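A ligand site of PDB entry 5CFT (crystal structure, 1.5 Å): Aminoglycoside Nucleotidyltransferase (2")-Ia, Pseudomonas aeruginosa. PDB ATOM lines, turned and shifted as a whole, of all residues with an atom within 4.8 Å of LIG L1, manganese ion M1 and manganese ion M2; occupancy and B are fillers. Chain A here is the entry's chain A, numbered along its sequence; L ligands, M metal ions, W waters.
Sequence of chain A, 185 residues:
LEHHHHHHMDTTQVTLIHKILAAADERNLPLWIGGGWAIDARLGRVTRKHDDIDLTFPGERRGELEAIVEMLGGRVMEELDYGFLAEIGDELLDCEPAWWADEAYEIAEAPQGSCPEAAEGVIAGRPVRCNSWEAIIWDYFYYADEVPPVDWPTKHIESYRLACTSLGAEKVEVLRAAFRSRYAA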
ATOM      1  N   GLY A  35     -17.526  25.212 -17.439  1.00  0.00           N
ATOM      2  CA  GLY A  35     -17.557  24.253 -18.506  1.00  0.00           C
ATOM      3  C   GLY A  35     -18.682  23.240 -18.479  1.00  0.00           C
ATOM      4  O   GLY A  35     -19.805  23.535 -18.082  1.00  0.00           O
ATOM      5  N   GLY A  36     -18.369  21.997 -18.849  1.00  0.00           N
ATOM      6  CA  GLY A  36     -19.382  20.961 -18.997  1.00  0.00           C
ATOM      7  C   GLY A  36     -20.123  20.668 -17.735  1.00  0.00           C
ATOM      8  O   GLY A  36     -21.324  20.443 -17.734  1.00  0.00           O
ATOM      9  N   TRP A  37     -19.395  20.571 -16.617  1.00  0.00           N
ATOM     10  CA  TRP A  37     -20.059  20.340 -15.353  1.00  0.00           C
ATOM     11  C   TRP A  37     -20.929  21.516 -14.926  1.00  0.00           C
ATOM     12  O   TRP A  37     -21.881  21.327 -14.210  1.00  0.00           O
ATOM     13  CB  TRP A  37     -19.061  19.980 -14.248  1.00  0.00           C
ATOM     14  CG  TRP A  37     -18.811  18.535 -14.078  1.00  0.00           C
ATOM     15  CD1 TRP A  37     -17.635  17.855 -14.342  1.00  0.00           C
ATOM     16  CD2 TRP A  37     -19.742  17.577 -13.628  1.00  0.00           C
ATOM     17  NE1 TRP A  37     -17.811  16.507 -14.071  1.00  0.00           N
ATOM     18  CE2 TRP A  37     -19.080  16.321 -13.576  1.00  0.00           C
ATOM     19  CE3 TRP A  37     -21.061  17.680 -13.191  1.00  0.00           C
ATOM     20  CZ2 TRP A  37     -19.753  15.147 -13.172  1.00  0.00           C
ATOM     21  CZ3 TRP A  37     -21.734  16.504 -12.777  1.00  0.00           C
ATOM     22  CH2 TRP A  37     -21.066  15.265 -12.772  1.00  0.00           C
ATOM     23  N   ARG A  48     -23.803  13.661 -19.774  1.00  0.00           N
ATOM     24  CA  ARG A  48     -22.781  12.890 -20.446  1.00  0.00           C
ATOM     25  C   ARG A  48     -21.594  12.753 -19.519  1.00  0.00           C
ATOM     26  O   ARG A  48     -21.520  13.396 -18.469  1.00  0.00           O
ATOM     27  CB  ARG A  48     -22.354  13.549 -21.758  1.00  0.00           C
ATOM     28  CG  ARG A  48     -21.797  14.968 -21.599  1.00  0.00           C
ATOM     29  CD  ARG A  48     -21.282  15.429 -22.946  1.00  0.00           C
ATOM     30  NE  ARG A  48     -20.758  16.785 -22.962  1.00  0.00           N
ATOM     31  CZ  ARG A  48     -19.532  17.163 -22.588  1.00  0.00           C
ATOM     32  NH1 ARG A  48     -19.165  18.416 -22.659  1.00  0.00           N
ATOM     33  NH2 ARG A  48     -18.656  16.288 -22.082  1.00  0.00           N
ATOM     34  N   LYS A  49     -20.645  11.911 -19.931  1.00  0.00           N
ATOM     35  CA  LYS A  49     -19.336  11.811 -19.279  1.00  0.00           C
ATOM     36  C   LYS A  49     -18.576  13.112 -19.515  1.00  0.00           C
ATOM     37  O   LYS A  49     -18.659  13.680 -20.590  1.00  0.00           O
ATOM     38  CB  LYS A  49     -18.593  10.604 -19.847  1.00  0.00           C
ATOM     39  CG  LYS A  49     -19.244   9.299 -19.477  1.00  0.00           C
ATOM     40  N   HIS A  50     -17.832  13.555 -18.508  1.00  0.00           N
ATOM     41  CA  HIS A  50     -17.054  14.776 -18.565  1.00  0.00           C
ATOM     42  C   HIS A  50     -15.569  14.440 -18.493  1.00  0.00           C
ATOM     43  O   HIS A  50     -15.138  13.698 -17.616  1.00  0.00           O
ATOM     44  CB  HIS A  50     -17.432  15.666 -17.408  1.00  0.00           C
ATOM     45  CG  HIS A  50     -18.857  16.145 -17.492  1.00  0.00           C
ATOM     46  ND1 HIS A  50     -19.239  17.019 -18.466  1.00  0.00           N
ATOM     47  CD2 HIS A  50     -19.988  15.766 -16.847  1.00  0.00           C
ATOM     48  CE1 HIS A  50     -20.541  17.229 -18.384  1.00  0.00           C
ATOM     49  NE2 HIS A  50     -21.011  16.487 -17.405  1.00  0.00           N
ATOM     50  N   ASP A  51     -14.797  15.053 -19.378  1.00  0.00           N
ATOM     51  CA  ASP A  51     -13.376  14.724 -19.458  1.00  0.00           C
ATOM     52  C   ASP A  51     -12.534  15.349 -18.364  1.00  0.00           C
ATOM     53  O   ASP A  51     -11.487  14.814 -17.994  1.00  0.00           O
ATOM     54  CB  ASP A  51     -12.834  15.105 -20.820  1.00  0.00           C
ATOM     55  CG  ASP A  51     -13.268  14.132 -21.919  1.00  0.00           C
ATOM     56  OD1 ASP A  51     -13.857  13.072 -21.614  1.00  0.00           O
ATOM     57  OD2 ASP A  51     -12.968  14.407 -23.092  1.00  0.00           O
ATOM     58  N   ASP A  52     -13.000  16.466 -17.828  1.00  0.00           N
ATOM     59  CA  ASP A  52     -12.309  17.146 -16.727  1.00  0.00           C
ATOM     60  C   ASP A  52     -13.282  17.920 -15.859  1.00  0.00           C
ATOM     61  O   ASP A  52     -14.495  17.858 -16.072  1.00  0.00           O
ATOM     62  CB  ASP A  52     -11.184  18.075 -17.248  1.00  0.00           C
ATOM     63  CG  ASP A  52     -11.662  19.204 -18.054  1.00  0.00           C
ATOM     64  OD1 ASP A  52     -12.824  19.558 -17.962  1.00  0.00           O
ATOM     65  OD2 ASP A  52     -10.800  19.820 -18.783  1.00  0.00           O
ATOM     66  N   ASP A  54     -13.671  21.799 -14.698  1.00  0.00           N
ATOM     67  CA  ASP A  54     -13.291  23.181 -14.866  1.00  0.00           C
ATOM     68  C   ASP A  54     -13.667  23.972 -13.625  1.00  0.00           C
ATOM     69  O   ASP A  54     -14.809  23.912 -13.174  1.00  0.00           O
ATOM     70  CB  ASP A  54     -13.971  23.747 -16.108  1.00  0.00           C
ATOM     71  CG  ASP A  54     -13.639  22.982 -17.365  1.00  0.00           C
ATOM     72  OD1 ASP A  54     -12.474  23.071 -17.850  1.00  0.00           O
ATOM     73  OD2 ASP A  54     -14.517  22.248 -17.889  1.00  0.00           O
ATOM     74  N   ASP A  94      -9.069  21.835 -14.424  1.00  0.00           N
ATOM     75  CA  ASP A  94      -8.650  22.889 -15.345  1.00  0.00           C
ATOM     76  C   ASP A  94      -9.035  24.196 -14.709  1.00  0.00           C
ATOM     77  O   ASP A  94     -10.241  24.508 -14.637  1.00  0.00           O
ATOM     78  CB  ASP A  94      -9.322  22.636 -16.680  1.00  0.00           C
ATOM     79  CG  ASP A  94      -9.013  23.644 -17.714  1.00  0.00           C
ATOM     80  OD1 ASP A  94      -8.248  24.578 -17.500  1.00  0.00           O
ATOM     81  OD2 ASP A  94      -9.519  23.448 -18.852  1.00  0.00           O
ATOM     82  N   ILE A 136     -20.392  30.876 -19.528  1.00  0.00           N
ATOM     83  CA  ILE A 136     -20.258  29.563 -20.170  1.00  0.00           C
ATOM     84  C   ILE A 136     -20.288  29.697 -21.672  1.00  0.00           C
ATOM     85  O   ILE A 136     -19.441  29.184 -22.381  1.00  0.00           O
ATOM     86  CB  ILE A 136     -21.342  28.626 -19.659  1.00  0.00           C
ATOM     87  CG1 ILE A 136     -21.148  28.285 -18.172  1.00  0.00           C
ATOM     88  CG2 ILE A 136     -21.354  27.344 -20.533  1.00  0.00           C
ATOM     89  CD1 ILE A 136     -22.343  27.611 -17.604  1.00  0.00           C
ATOM     90  N   ASP A 139     -17.271  31.561 -23.461  1.00  0.00           N
ATOM     91  CA  ASP A 139     -16.077  30.769 -23.787  1.00  0.00           C
ATOM     92  C   ASP A 139     -16.251  29.958 -25.054  1.00  0.00           C
ATOM     93  O   ASP A 139     -15.273  29.703 -25.731  1.00  0.00           O
ATOM     94  CB  ASP A 139     -15.677  29.858 -22.616  1.00  0.00           C
ATOM     95  CG  ASP A 139     -14.598  30.428 -21.741  1.00  0.00           C
ATOM     96  OD1 ASP A 139     -14.030  31.474 -22.090  1.00  0.00           O
ATOM     97  OD2 ASP A 139     -14.331  29.763 -20.710  1.00  0.00           O
ATOM     98  N   TYR A 140     -17.477  29.603 -25.423  1.00  0.00           N
ATOM     99  CA  TYR A 140     -17.693  28.979 -26.717  1.00  0.00           C
ATOM    100  C   TYR A 140     -17.499  29.933 -27.866  1.00  0.00           C
ATOM    101  O   TYR A 140     -17.126  29.515 -28.964  1.00  0.00           O
ATOM    102  CB  TYR A 140     -19.115  28.355 -26.837  1.00  0.00           C
ATOM    103  CG  TYR A 140     -19.330  27.066 -26.128  1.00  0.00           C
ATOM    104  CD1 TYR A 140     -18.977  25.864 -26.693  1.00  0.00           C
ATOM    105  CD2 TYR A 140     -19.933  27.026 -24.887  1.00  0.00           C
ATOM    106  CE1 TYR A 140     -19.213  24.671 -26.008  1.00  0.00           C
ATOM    107  CE2 TYR A 140     -20.164  25.869 -24.225  1.00  0.00           C
ATOM    108  CZ  TYR A 140     -19.783  24.680 -24.808  1.00  0.00           C
ATOM    109  OH  TYR A 140     -20.015  23.493 -24.111  1.00  0.00           O
ATOM    110  N   TYR A 143     -13.912  29.799 -28.522  1.00  0.00           N
ATOM    111  CA  TYR A 143     -13.657  28.502 -29.158  1.00  0.00           C
ATOM    112  C   TYR A 143     -13.996  28.601 -30.654  1.00  0.00           C
ATOM    113  O   TYR A 143     -13.231  28.100 -31.495  1.00  0.00           O
ATOM    114  CB  TYR A 143     -14.482  27.451 -28.459  1.00  0.00           C
ATOM    115  CG  TYR A 143     -14.310  25.992 -28.813  1.00  0.00           C
ATOM    116  CD1 TYR A 143     -13.171  25.531 -29.393  1.00  0.00           C
ATOM    117  CD2 TYR A 143     -15.315  25.084 -28.478  1.00  0.00           C
ATOM    118  CE1 TYR A 143     -13.021  24.175 -29.687  1.00  0.00           C
ATOM    119  CE2 TYR A 143     -15.183  23.758 -28.766  1.00  0.00           C
ATOM    120  CZ  TYR A 143     -14.043  23.323 -29.362  1.00  0.00           C
ATOM    121  OH  TYR A 143     -13.881  21.963 -29.615  1.00  0.00           O
ATOM    122  N   GLU A 146     -11.399  29.908 -32.689  1.00  0.00           N
ATOM    123  CA  GLU A 146     -10.305  28.937 -32.837  1.00  0.00           C
ATOM    124  C   GLU A 146     -10.698  27.721 -33.687  1.00  0.00           C
ATOM    125  O   GLU A 146      -9.832  27.100 -34.304  1.00  0.00           O
ATOM    126  CB  GLU A 146      -9.829  28.482 -31.457  1.00  0.00           C
ATOM    127  CG  GLU A 146      -9.336  29.623 -30.548  1.00  0.00           C
ATOM    128  CD  GLU A 146      -8.149  30.329 -31.141  1.00  0.00           C
ATOM    129  OE1 GLU A 146      -7.396  29.682 -31.908  1.00  0.00           O
ATOM    130  OE2 GLU A 146      -7.968  31.542 -30.867  1.00  0.00           O
ATOM    131  N   HIS A 156     -19.321  18.705 -27.911  1.00  0.00           N
ATOM    132  CA  HIS A 156     -19.200  20.134 -27.649  1.00  0.00           C
ATOM    133  C   HIS A 156     -20.320  20.883 -28.327  1.00  0.00           C
ATOM    134  O   HIS A 156     -20.803  21.901 -27.820  1.00  0.00           O
ATOM    135  CB  HIS A 156     -17.853  20.693 -28.093  1.00  0.00           C
ATOM    136  CG  HIS A 156     -16.697  20.160 -27.332  1.00  0.00           C
ATOM    137  ND1 HIS A 156     -15.394  20.270 -27.760  1.00  0.00           N
ATOM    138  CD2 HIS A 156     -16.648  19.464 -26.160  1.00  0.00           C
ATOM    139  CE1 HIS A 156     -14.591  19.691 -26.895  1.00  0.00           C
ATOM    140  NE2 HIS A 156     -15.318  19.176 -25.929  1.00  0.00           N
HETATM  141  P1  LIG L   1     -16.098  18.148 -20.563  1.00  0.00           P
HETATM  142  O1  LIG L   1     -16.082  16.771 -21.322  1.00  0.00           O
HETATM  143  O2  LIG L   1     -14.701  18.574 -20.186  1.00  0.00           O
HETATM  144  O3  LIG L   1     -17.076  18.239 -19.520  1.00  0.00           O
HETATM  145  P2  LIG L   1     -16.241  20.727 -21.708  1.00  0.00           P
HETATM  146  O4  LIG L   1     -17.368  21.492 -22.444  1.00  0.00           O
HETATM  147  O5  LIG L   1     -16.002  21.202 -20.299  1.00  0.00           O
HETATM  148  O6  LIG L   1     -16.646  19.221 -21.645  1.00  0.00           O
HETATM  149  P3  LIG L   1     -13.338  21.549 -22.169  1.00  0.00           P
HETATM  150  O7  LIG L   1     -12.098  21.253 -22.980  1.00  0.00           O
HETATM  151  O8  LIG L   1     -13.117  21.349 -20.664  1.00  0.00           O
HETATM  152  C1  LIG L   1     -14.758  20.651 -22.696  1.00  0.00           C
HETATM  153  O9  LIG L   1     -13.529  23.098 -22.389  1.00  0.00           O
HETATM  154  C2  LIG L   1     -14.090  24.031 -21.432  1.00  0.00           C
HETATM  155  C3  LIG L   1     -14.683  25.114 -22.279  1.00  0.00           C
HETATM  156  O10 LIG L   1     -13.636  25.725 -23.066  1.00  0.00           O
HETATM  157  C4  LIG L   1     -15.674  24.556 -23.272  1.00  0.00           C
HETATM  158  O11 LIG L   1     -16.932  24.592 -22.602  1.00  0.00           O
HETATM  159  C5  LIG L   1     -15.538  25.492 -24.466  1.00  0.00           C
HETATM  160  O12 LIG L   1     -16.352  26.613 -24.140  1.00  0.00           O
HETATM  161  C6  LIG L   1     -14.045  25.866 -24.423  1.00  0.00           C
HETATM  162  N1  LIG L   1     -13.135  25.106 -25.319  1.00  0.00           N
HETATM  163  C7  LIG L   1     -13.053  23.761 -25.551  1.00  0.00           C
HETATM  164  N2  LIG L   1     -12.009  23.399 -26.268  1.00  0.00           N
HETATM  165  C8  LIG L   1     -11.383  24.597 -26.556  1.00  0.00           C
HETATM  166  C9  LIG L   1     -10.284  24.915 -27.377  1.00  0.00           C
HETATM  167  N3  LIG L   1      -9.533  24.001 -28.011  1.00  0.00           N
HETATM  168  N4  LIG L   1      -9.977  26.220 -27.551  1.00  0.00           N
HETATM  169  C10 LIG L   1     -10.706  27.135 -26.927  1.00  0.00           C
HETATM  170  N5  LIG L   1     -11.758  26.956 -26.119  1.00  0.00           N
HETATM  171  C11 LIG L   1     -12.060  25.667 -25.983  1.00  0.00           C
HETATM  172  O1  LG2 L   2     -10.415  22.737 -21.491  1.00  0.00           O
HETATM  173  C1  LG2 L   2      -9.649  23.361 -22.526  1.00  0.00           C
HETATM  174  C2  LG2 L   2      -8.163  23.324 -22.184  1.00  0.00           C
HETATM  175  N1  LG2 L   2      -7.679  21.961 -21.993  1.00  0.00           N
HETATM  176  C3  LG2 L   2      -6.901  21.792 -20.765  1.00  0.00           C
HETATM  177  C4  LG2 L   2      -7.372  23.966 -23.317  1.00  0.00           C
HETATM  178  C5  LG2 L   2      -5.893  24.071 -22.978  1.00  0.00           C
HETATM  179  O2  LG2 L   2      -7.510  23.072 -24.435  1.00  0.00           O
HETATM  180  C6  LG2 L   2      -7.938  25.361 -23.626  1.00  0.00           C
HETATM  181  O3  LG2 L   2      -9.353  25.341 -23.814  1.00  0.00           O
HETATM  182  C7  LG2 L   2     -10.114  24.791 -22.755  1.00  0.00           C
HETATM  183  O4  LG2 L   2      -9.866  25.566 -21.616  1.00  0.00           O
HETATM  184  C8  LG2 L   2     -10.678  26.748 -21.370  1.00  0.00           C
HETATM  185  C9  LG2 L   2     -10.699  26.982 -19.860  1.00  0.00           C
HETATM  186  N2  LG2 L   2     -11.209  25.832 -19.081  1.00  0.00           N
HETATM  187  C10 LG2 L   2     -11.511  28.243 -19.549  1.00  0.00           C
HETATM  188  C11 LG2 L   2     -10.921  29.476 -20.259  1.00  0.00           C
HETATM  189  N3  LG2 L   2     -11.730  30.674 -19.929  1.00  0.00           N
HETATM  190  C12 LG2 L   2     -10.079  27.953 -22.075  1.00  0.00           C
HETATM  191  O5  LG2 L   2     -10.158  27.799 -23.501  1.00  0.00           O
HETATM  192  C13 LG2 L   2     -10.820  29.242 -21.747  1.00  0.00           C
HETATM  193  O6  LG2 L   2     -10.034  30.325 -22.277  1.00  0.00           O
HETATM  194  C14 LG2 L   2     -10.712  31.370 -22.940  1.00  0.00           C
HETATM  195  C15 LG2 L   2     -10.099  31.605 -24.327  1.00  0.00           C
HETATM  196  N4  LG2 L   2     -10.051  30.361 -25.091  1.00  0.00           N
HETATM  197  C16 LG2 L   2      -8.694  32.117 -24.117  1.00  0.00           C
HETATM  198  C17 LG2 L   2      -8.779  33.392 -23.298  1.00  0.00           C
HETATM  199  O7  LG2 L   2     -10.757  32.555 -22.178  1.00  0.00           O
HETATM  200  C18 LG2 L   2      -9.454  33.153 -21.964  1.00  0.00           C
HETATM  201  C19 LG2 L   2      -9.687  34.403 -21.153  1.00  0.00           C
HETATM  202  C20 LG2 L   2     -10.447  35.439 -21.962  1.00  0.00           C
HETATM  203  N5  LG2 L   2     -10.400  34.098 -19.904  1.00  0.00           N
HETATM  204  C21 LG2 L   2     -10.382  35.205 -18.971  1.00  0.00           C
HETATM  205 MN    MN M   1     -14.330  20.537 -19.074  1.00  0.00          MN
HETATM  206 MN    MN M   2     -11.244  22.019 -19.426  1.00  0.00          MN
HETATM  207  O   HOH W   1     -12.721  29.184 -24.824  1.00  0.00           O
HETATM  208  O   HOH W   2     -17.962  26.973 -21.442  1.00  0.00           O
HETATM  209  O   HOH W   3     -12.291  18.208 -21.381  1.00  0.00           O
HETATM  210  O   HOH W   4     -14.612  16.964 -23.736  1.00  0.00           O
HETATM  211  O   HOH W   5     -11.628  20.045 -25.294  1.00  0.00           O
HETATM  212  O   HOH W   6      -9.332  19.991 -22.789  1.00  0.00           O
HETATM  213  O   HOH W   7     -15.862  19.606 -17.666  1.00  0.00           O
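O3 of LIG L1 is in hydrogen-bond range of ND1 of His 50 (2.7 Å).
NH2 of Arg 48 lies within salt-bridge range of O1 of LIG L1, 2.7 Å away.
The backbone NH (N) of Gly 36 sits close to an oxygen (O5) of LIG L1 (2.9 Å).
The backbone NH (N) of Asp 51 lies within hydrogen-bond range of an oxygen (O1) of LIG L1, 2.9 Å away.
N of Tyr 140 sits at hydrogen-bond distance from O12 of LIG L1.
The side-chain carboxylate (OD2) of Asp 139 lies within salt-bridge range of a nitrogen (N3) of LG2 L2 (2.9 Å).
NE2 of His 50 lies close to O of Arg 48, at 3.3 Å.
A ring nitrogen (ND1) of His 156 sits at hydrogen-bond distance from the side-chain hydroxyl (OH) of Tyr 143 (2.9 Å).
Merely in contact with LIG L1: Asp 139, Tyr 143, His 156 and Gly 35.
11 residues have an atom within 4 Å of LIG L1: Gly 35, Gly 36, Arg 48, His 50, Asp 51, Asp 52, Asp 54, Asp 139, Tyr 140, Tyr 143 and His 156.
Along chain A the residues within 4 Å of LIG L1 span positions 35 to 156.
Within 4 Å of manganese ion M1: Asp 52 and Asp 54.
The nearest printed residue that does not touch manganese ion M1 is Gly 36 (4.3 Å).
Three residues have an atom within 4 Å of manganese ion M2: Asp 52, Asp 54 and Asp 94.
The nearest printed residue that does not touch manganese ion M2 is Gly 35 (6.8 Å).
Manganese ion M1 is bound by OD2 of Asp 54 (2.1 Å), OD1 of Asp 52 (2.1 Å), O8 of LIG L1 (2.2 Å), O5 of LIG L1 (2.2 Å), water W7 (2.3 Å) and O2 of LIG L1 (2.3 Å).
Manganese ion M2 is bound by OD1 of Asp 54 (2.3 Å).
Manganese ion M2 is bound by OD2 of Asp 94 (2.3 Å).
OD2 of Asp 52 binds manganese ion M2 (2.3 Å).
O1 of LG2 L2 binds manganese ion M2 (2.3 Å).
Manganese ion M2 is bound by an oxygen (O8) of LIG L1, 2.3 Å away.
Manganese ion M2 has five donor atoms within binding distance.
Water W7 bridges O3 of LIG L1 (2.6 Å) and O of Asp 52 (2.7 Å).
Water W1 lies within hydrogen-bond range of a nitrogen (N5) of LIG L1 (2.8 Å), the backbone carbonyl oxygen (O) of Asp 139 (2.8 Å) and a nitrogen (N4) of LG2 L2 (2.9 Å).
Water W4 lies within hydrogen-bond range of an oxygen (O1) of LIG L1 (2.8 Å), the side-chain carboxylate (OD2) of Asp 51 (3.1 Å) and a ring nitrogen (NE2) of His 156 (3.2 Å).
Water W2 bridges the backbone carbonyl oxygen of Ile 136 (2.8 Å) and an oxygen (O11) of LIG L1 (2.8 Å).
Water W6 bridges N1 of LG2 L2 and O7 of LIG L1.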
